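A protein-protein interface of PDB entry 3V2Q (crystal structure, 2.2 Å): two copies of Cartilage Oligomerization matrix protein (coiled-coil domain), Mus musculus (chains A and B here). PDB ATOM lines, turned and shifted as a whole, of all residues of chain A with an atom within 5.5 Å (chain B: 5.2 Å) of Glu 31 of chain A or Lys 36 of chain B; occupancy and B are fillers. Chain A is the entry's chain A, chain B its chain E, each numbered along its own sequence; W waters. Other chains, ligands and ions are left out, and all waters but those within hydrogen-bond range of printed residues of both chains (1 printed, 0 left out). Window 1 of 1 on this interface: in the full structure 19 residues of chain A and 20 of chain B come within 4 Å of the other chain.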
ATOM      1  N   GLN A  27     -16.971  29.950 -22.962  1.00  0.00           N
ATOM      2  CA  GLN A  27     -15.715  29.498 -22.388  1.00  0.00           C
ATOM      3  C   GLN A  27     -15.154  28.296 -23.157  1.00  0.00           C
ATOM      4  O   GLN A  27     -13.945  28.223 -23.410  1.00  0.00           O
ATOM      5  CB  GLN A  27     -15.923  29.117 -20.919  1.00  0.00           C
ATOM      6  CG  GLN A  27     -14.746  28.396 -20.284  1.00  0.00           C
ATOM      7  CD  GLN A  27     -13.451  29.179 -20.393  1.00  0.00           C
ATOM      8  OE1 GLN A  27     -13.347  30.309 -19.906  1.00  0.00           O
ATOM      9  NE2 GLN A  27     -12.457  28.581 -21.036  1.00  0.00           N
ATOM     10  N   GLN A  28     -16.028  27.361 -23.523  1.00  0.00           N
ATOM     11  CA  GLN A  28     -15.597  26.166 -24.240  1.00  0.00           C
ATOM     12  C   GLN A  28     -14.865  26.535 -25.519  1.00  0.00           C
ATOM     13  O   GLN A  28     -13.793  26.010 -25.796  1.00  0.00           O
ATOM     14  CB  GLN A  28     -16.798  25.262 -24.556  1.00  0.00           C
ATOM     15  CG  GLN A  28     -16.448  23.972 -25.292  1.00  0.00           C
ATOM     16  CD  GLN A  28     -17.588  22.953 -25.291  1.00  0.00           C
ATOM     17  OE1 GLN A  28     -17.671  22.094 -24.404  1.00  0.00           O
ATOM     18  NE2 GLN A  28     -18.476  23.053 -26.275  1.00  0.00           N
ATOM     19  N   VAL A  29     -15.448  27.444 -26.286  1.00  0.00           N
ATOM     20  CA  VAL A  29     -14.857  27.902 -27.535  1.00  0.00           C
ATOM     21  C   VAL A  29     -13.435  28.426 -27.305  1.00  0.00           C
ATOM     22  O   VAL A  29     -12.537  28.162 -28.094  1.00  0.00           O
ATOM     23  CB  VAL A  29     -15.733  29.011 -28.163  1.00  0.00           C
ATOM     24  CG1 VAL A  29     -15.002  29.677 -29.318  1.00  0.00           C
ATOM     25  CG2 VAL A  29     -17.053  28.412 -28.637  1.00  0.00           C
ATOM     26  N   LYS A  30     -13.227  29.157 -26.215  1.00  0.00           N
ATOM     27  CA  LYS A  30     -11.899  29.683 -25.920  1.00  0.00           C
ATOM     28  C   LYS A  30     -10.918  28.557 -25.618  1.00  0.00           C
ATOM     29  O   LYS A  30      -9.781  28.579 -26.090  1.00  0.00           O
ATOM     30  CB  LYS A  30     -11.970  30.665 -24.753  1.00  0.00           C
ATOM     31  CG  LYS A  30     -12.875  31.853 -25.056  1.00  0.00           C
ATOM     32  CD  LYS A  30     -13.086  32.766 -23.859  1.00  0.00           C
ATOM     33  CE  LYS A  30     -14.117  33.847 -24.195  1.00  0.00           C
ATOM     34  NZ  LYS A  30     -14.477  34.687 -23.017  1.00  0.00           N
ATOM     35  N   GLU A  31     -11.346  27.565 -24.842  1.00  0.00           N
ATOM     36  CA  GLU A  31     -10.464  26.447 -24.531  1.00  0.00           C
ATOM     37  C   GLU A  31     -10.104  25.722 -25.829  1.00  0.00           C
ATOM     38  O   GLU A  31      -8.965  25.296 -26.028  1.00  0.00           O
ATOM     39  CB  GLU A  31     -11.148  25.470 -23.572  1.00  0.00           C
ATOM     40  CG  GLU A  31     -11.476  26.040 -22.203  1.00  0.00           C
ATOM     41  CD  GLU A  31     -10.242  26.449 -21.420  1.00  0.00           C
ATOM     42  OE1 GLU A  31      -9.271  25.666 -21.369  1.00  0.00           O
ATOM     43  OE2 GLU A  31     -10.249  27.548 -20.840  1.00  0.00           O
ATOM     44  N   ILE A  32     -11.083  25.583 -26.715  1.00  0.00           N
ATOM     45  CA  ILE A  32     -10.844  24.909 -27.986  1.00  0.00           C
ATOM     46  C   ILE A  32      -9.914  25.721 -28.890  1.00  0.00           C
ATOM     47  O   ILE A  32      -8.994  25.172 -29.492  1.00  0.00           O
ATOM     48  CB  ILE A  32     -12.168  24.638 -28.732  1.00  0.00           C
ATOM     49  CG1 ILE A  32     -12.915  23.496 -28.041  1.00  0.00           C
ATOM     50  CG2 ILE A  32     -11.891  24.311 -30.189  1.00  0.00           C
ATOM     51  CD1 ILE A  32     -14.292  23.223 -28.598  1.00  0.00           C
ATOM     52  N   THR A  33     -10.167  27.021 -28.991  1.00  0.00           N
ATOM     53  CA  THR A  33      -9.335  27.883 -29.817  1.00  0.00           C
ATOM     54  C   THR A  33      -7.913  27.845 -29.283  1.00  0.00           C
ATOM     55  O   THR A  33      -6.954  28.045 -30.024  1.00  0.00           O
ATOM     56  CB  THR A  33      -9.835  29.335 -29.795  1.00  0.00           C
ATOM     57  OG1 THR A  33     -11.167  29.387 -30.313  1.00  0.00           O
ATOM     58  CG2 THR A  33      -8.941  30.219 -30.647  1.00  0.00           C
ATOM     59  N   PHE A  34      -7.783  27.584 -27.987  1.00  0.00           N
ATOM     60  CA  PHE A  34      -6.479  27.507 -27.352  1.00  0.00           C
ATOM     61  C   PHE A  34      -5.818  26.184 -27.733  1.00  0.00           C
ATOM     62  O   PHE A  34      -4.631  26.131 -28.053  1.00  0.00           O
ATOM     63  CB  PHE A  34      -6.638  27.606 -25.833  1.00  0.00           C
ATOM     64  CG  PHE A  34      -5.341  27.565 -25.088  1.00  0.00           C
ATOM     65  CD1 PHE A  34      -4.624  26.375 -24.974  1.00  0.00           C
ATOM     66  CD2 PHE A  34      -4.809  28.723 -24.534  1.00  0.00           C
ATOM     67  CE1 PHE A  34      -3.398  26.341 -24.321  1.00  0.00           C
ATOM     68  CE2 PHE A  34      -3.582  28.698 -23.880  1.00  0.00           C
ATOM     69  CZ  PHE A  34      -2.874  27.504 -23.775  1.00  0.00           C
ATOM     70  N   LEU A  35      -6.599  25.113 -27.690  1.00  0.00           N
ATOM     71  CA  LEU A  35      -6.107  23.791 -28.042  1.00  0.00           C
ATOM     72  C   LEU A  35      -5.587  23.836 -29.479  1.00  0.00           C
ATOM     73  O   LEU A  35      -4.553  23.251 -29.799  1.00  0.00           O
ATOM     74  CB  LEU A  35      -7.252  22.778 -27.920  1.00  0.00           C
ATOM     75  CG  LEU A  35      -7.006  21.286 -28.169  1.00  0.00           C
ATOM     76  CD1 LEU A  35      -6.076  20.707 -27.098  1.00  0.00           C
ATOM     77  CD2 LEU A  35      -8.338  20.558 -28.149  1.00  0.00           C
ATOM     78  N   LYS A  36      -6.306  24.548 -30.340  1.00  0.00           N
ATOM     79  CA  LYS A  36      -5.920  24.665 -31.740  1.00  0.00           C
ATOM     80  C   LYS A  36      -4.561  25.322 -31.893  1.00  0.00           C
ATOM     81  O   LYS A  36      -3.698  24.817 -32.609  1.00  0.00           O
ATOM     82  CB  LYS A  36      -6.950  25.481 -32.520  1.00  0.00           C
ATOM     83  CG  LYS A  36      -6.599  25.638 -33.995  1.00  0.00           C
ATOM     84  CD  LYS A  36      -7.532  26.605 -34.705  1.00  0.00           C
ATOM     85  CE  LYS A  36      -7.385  28.017 -34.167  1.00  0.00           C
ATOM     86  NZ  LYS A  36      -8.252  28.967 -34.913  1.00  0.00           N
ATOM     87  N   GLU B  31     -13.678  18.231 -19.496  1.00  0.00           N
ATOM     88  CA  GLU B  31     -12.899  17.274 -20.288  1.00  0.00           C
ATOM     89  C   GLU B  31     -12.018  18.015 -21.299  1.00  0.00           C
ATOM     90  O   GLU B  31     -10.828  17.734 -21.429  1.00  0.00           O
ATOM     91  CB  GLU B  31     -13.840  16.309 -21.032  1.00  0.00           C
ATOM     92  CG  GLU B  31     -14.742  15.478 -20.117  1.00  0.00           C
ATOM     93  CD  GLU B  31     -14.036  14.281 -19.502  1.00  0.00           C
ATOM     94  OE1 GLU B  31     -12.888  14.421 -19.044  1.00  0.00           O
ATOM     95  OE2 GLU B  31     -14.639  13.189 -19.464  1.00  0.00           O
ATOM     96  N   ILE B  32     -12.604  18.963 -22.013  1.00  0.00           N
ATOM     97  CA  ILE B  32     -11.842  19.728 -22.982  1.00  0.00           C
ATOM     98  C   ILE B  32     -10.681  20.447 -22.290  1.00  0.00           C
ATOM     99  O   ILE B  32      -9.550  20.411 -22.784  1.00  0.00           O
ATOM    100  CB  ILE B  32     -12.747  20.739 -23.716  1.00  0.00           C
ATOM    101  CG1 ILE B  32     -13.658  19.975 -24.685  1.00  0.00           C
ATOM    102  CG2 ILE B  32     -11.895  21.791 -24.431  1.00  0.00           C
ATOM    103  CD1 ILE B  32     -14.765  20.803 -25.279  1.00  0.00           C
ATOM    104  N   THR B  33     -10.954  21.081 -21.149  1.00  0.00           N
ATOM    105  CA  THR B  33      -9.902  21.772 -20.406  1.00  0.00           C
ATOM    106  C   THR B  33      -8.806  20.786 -19.989  1.00  0.00           C
ATOM    107  O   THR B  33      -7.633  21.146 -19.935  1.00  0.00           O
ATOM    108  CB  THR B  33     -10.461  22.469 -19.143  1.00  0.00           C
ATOM    109  OG1 THR B  33     -11.328  23.543 -19.529  1.00  0.00           O
ATOM    110  CG2 THR B  33      -9.332  23.032 -18.302  1.00  0.00           C
ATOM    111  N   PHE B  34      -9.189  19.546 -19.696  1.00  0.00           N
ATOM    112  CA  PHE B  34      -8.223  18.519 -19.309  1.00  0.00           C
ATOM    113  C   PHE B  34      -7.379  18.100 -20.509  1.00  0.00           C
ATOM    114  O   PHE B  34      -6.171  17.907 -20.392  1.00  0.00           O
ATOM    115  CB  PHE B  34      -8.941  17.295 -18.732  1.00  0.00           C
ATOM    116  CG  PHE B  34      -9.624  17.554 -17.417  1.00  0.00           C
ATOM    117  CD1 PHE B  34      -9.231  18.621 -16.608  1.00  0.00           C
ATOM    118  CD2 PHE B  34     -10.626  16.701 -16.960  1.00  0.00           C
ATOM    119  CE1 PHE B  34      -9.823  18.831 -15.364  1.00  0.00           C
ATOM    120  CE2 PHE B  34     -11.224  16.899 -15.717  1.00  0.00           C
ATOM    121  CZ  PHE B  34     -10.822  17.966 -14.915  1.00  0.00           C
ATOM    122  N   LEU B  35      -8.020  17.950 -21.664  1.00  0.00           N
ATOM    123  CA  LEU B  35      -7.306  17.585 -22.884  1.00  0.00           C
ATOM    124  C   LEU B  35      -6.321  18.711 -23.232  1.00  0.00           C
ATOM    125  O   LEU B  35      -5.180  18.459 -23.628  1.00  0.00           O
ATOM    126  CB  LEU B  35      -8.303  17.381 -24.027  1.00  0.00           C
ATOM    127  CG  LEU B  35      -7.758  17.040 -25.419  1.00  0.00           C
ATOM    128  CD1 LEU B  35      -6.975  15.723 -25.395  1.00  0.00           C
ATOM    129  CD2 LEU B  35      -8.931  16.950 -26.384  1.00  0.00           C
ATOM    130  N   LYS B  36      -6.770  19.954 -23.072  1.00  0.00           N
ATOM    131  CA  LYS B  36      -5.939  21.117 -23.345  1.00  0.00           C
ATOM    132  C   LYS B  36      -4.696  21.094 -22.460  1.00  0.00           C
ATOM    133  O   LYS B  36      -3.577  21.266 -22.941  1.00  0.00           O
ATOM    134  CB  LYS B  36      -6.720  22.403 -23.070  1.00  0.00           C
ATOM    135  CG  LYS B  36      -5.908  23.679 -23.268  1.00  0.00           C
ATOM    136  CD  LYS B  36      -6.554  24.877 -22.584  1.00  0.00           C
ATOM    137  CE  LYS B  36      -6.563  24.716 -21.066  1.00  0.00           C
ATOM    138  NZ  LYS B  36      -7.153  25.902 -20.379  1.00  0.00           N
ATOM    139  N   ASN B  37      -4.891  20.894 -21.160  1.00  0.00           N
ATOM    140  CA  ASN B  37      -3.757  20.856 -20.249  1.00  0.00           C
ATOM    141  C   ASN B  37      -2.832  19.684 -20.571  1.00  0.00           C
ATOM    142  O   ASN B  37      -1.623  19.756 -20.355  1.00  0.00           O
ATOM    143  CB  ASN B  37      -4.231  20.767 -18.796  1.00  0.00           C
ATOM    144  CG  ASN B  37      -4.825  22.070 -18.300  1.00  0.00           C
ATOM    145  OD1 ASN B  37      -4.308  23.147 -18.591  1.00  0.00           O
ATOM    146  ND2 ASN B  37      -5.906  21.980 -17.539  1.00  0.00           N
ATOM    147  N   THR B  38      -3.404  18.613 -21.106  1.00  0.00           N
ATOM    148  CA  THR B  38      -2.633  17.428 -21.456  1.00  0.00           C
ATOM    149  C   THR B  38      -1.748  17.647 -22.677  1.00  0.00           C
ATOM    150  O   THR B  38      -0.581  17.256 -22.685  1.00  0.00           O
ATOM    151  CB  THR B  38      -3.565  16.234 -21.713  1.00  0.00           C
ATOM    152  OG1 THR B  38      -4.250  15.904 -20.499  1.00  0.00           O
ATOM    153  CG2 THR B  38      -2.771  15.021 -22.201  1.00  0.00           C
ATOM    154  N   VAL B  39      -2.308  18.275 -23.706  1.00  0.00           N
ATOM    155  CA  VAL B  39      -1.569  18.547 -24.931  1.00  0.00           C
ATOM    156  C   VAL B  39      -0.498  19.610 -24.697  1.00  0.00           C
ATOM    157  O   VAL B  39       0.546  19.601 -25.343  1.00  0.00           O
ATOM    158  CB  VAL B  39      -2.517  19.020 -26.047  1.00  0.00           C
ATOM    159  CG1 VAL B  39      -1.734  19.290 -27.320  1.00  0.00           C
ATOM    160  CG2 VAL B  39      -3.575  17.969 -26.295  1.00  0.00           C
ATOM    161  N   MET B  40      -0.763  20.525 -23.771  1.00  0.00           N
ATOM    162  CA  MET B  40       0.189  21.580 -23.450  1.00  0.00           C
ATOM    163  C   MET B  40       1.427  20.999 -22.780  1.00  0.00           C
ATOM    164  O   MET B  40       2.488  21.628 -22.762  1.00  0.00           O
ATOM    165  CB  MET B  40      -0.441  22.594 -22.503  1.00  0.00           C
ATOM    166  CG  MET B  40      -1.257  23.676 -23.167  1.00  0.00           C
ATOM    167  SD  MET B  40      -2.027  24.720 -21.920  1.00  0.00           S
ATOM    168  CE  MET B  40      -0.609  25.342 -21.060  1.00  0.00           C
ATOM    169  N   GLU B  41       1.281  19.798 -22.226  1.00  0.00           N
ATOM    170  CA  GLU B  41       2.372  19.126 -21.531  1.00  0.00           C
ATOM    171  C   GLU B  41       2.946  17.956 -22.325  1.00  0.00           C
ATOM    172  O   GLU B  41       3.855  17.267 -21.854  1.00  0.00           O
ATOM    173  CB  GLU B  41       1.881  18.621 -20.174  1.00  0.00           C
ATOM    174  CG  GLU B  41       1.207  19.686 -19.327  1.00  0.00           C
ATOM    175  CD  GLU B  41       2.108  20.874 -19.062  1.00  0.00           C
ATOM    176  OE1 GLU B  41       3.241  20.658 -18.583  1.00  0.00           O
ATOM    177  OE2 GLU B  41       1.686  22.020 -19.327  1.00  0.00           O
HETATM  178  O   HOH W   1      -8.487  26.750 -18.240  1.00  0.00           O
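The side-chain amide nitrogen of Gln 27 of chain A is in hydrogen-bond range of the side-chain carboxylate of Glu 31 of chain A. The backbone carbonyl oxygen (O) of Thr 33 of chain B lies within hydrogen-bond range of the side-chain amide nitrogen (ND2) of Asn 37 of chain B, 3.1 Å away.
Glu 31 of chain A touches Ile 32 of chain B, but with the chains exchanged Ile 32 of chain A does not touch Glu 31 of chain B (8.7 Å). Glu 31 of chain A touches Thr 33 of chain B, but with the chains exchanged Thr 33 of chain A does not touch Glu 31 of chain B (12.0 Å). Glu 31 of chain A touches Lys 36 of chain B, but with the chains exchanged Lys 36 of chain A does not touch Glu 31 of chain B (12.1 Å). Leu 35 of chain A touches Lys 36 of chain B, but with the chains exchanged Lys 36 of chain A does not touch Leu 35 of chain B (9.0 Å). Of the 8 pairs that touch across the chains among the printed residues, none has its exchanged pair printed and touching as well.
Glu 31 of chain A touches just these residues of chain B: Ile 32 (3.9 Å), Thr 33 (3.5 Å) and Lys 36 (2.3 Å). Printed residues of chain A within 4 Å of Thr 33 of chain B: Glu 31 (3.5 Å). Of the printed residues of chain A, Ile 32 of chain B touches Gln 28 and Glu 31. Printed residues of chain A within 4 Å of Val 39 of chain B: Leu 35 (3.8 Å). Printed residues of chain A within 4 Å of Met 40 of chain B: Phe 34 (3.2 Å). Thr 33 of chain A touches none of the printed residues of chain B. Glu 41 of chain B touches none of the printed residues of chain A. The nearest printed residue of chain A that does not touch Lys 36 of chain B is Gln 27 of chain A (6.0 Å). The nearest printed residue of chain A that does not touch Thr 33 of chain B is Gln 27 of chain A (5.4 Å).
Among the printed residues, pairs that only touch across the chains: Phe 34 of chain A with Met 40 of chain B, Gln 28 of chain A with Ile 32 of chain B, Phe 34 of chain A with Lys 36 of chain B, Leu 35 of chain A with Lys 36 of chain B, Leu 35 of chain A with Val 39 of chain B and Glu 31 of chain A with Ile 32 of chain B.
Of the 11 printed residues of chain B, 5 touch a printed residue of chain A. Hydrophobic or aromatic side chains of chain B within 4 Å of the printed part of chain A: Ile 32, Val 39 and Met 40. Of the 10 printed residues of chain A, 4 touch a printed residue of chain B. Hydrophobic or aromatic side chains of chain A within 4 Å of the printed part of chain B: Phe 34 and Leu 35.
OG1 of Thr 33 of chain B sits at hydrogen-bond distance from OE1 of Glu 31 of chain A, at 3.5 Å. The side-chain amino group (NZ) of Lys 36 of chain B is in salt-bridge range of the side-chain carboxylate (OE2) of Glu 31 of chain A, 3.5 Å away.
Water W1 bridges NZ of Lys 36 of chain B (2.7 Å) and OE2 of Glu 31 of chain A (3.2 Å).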
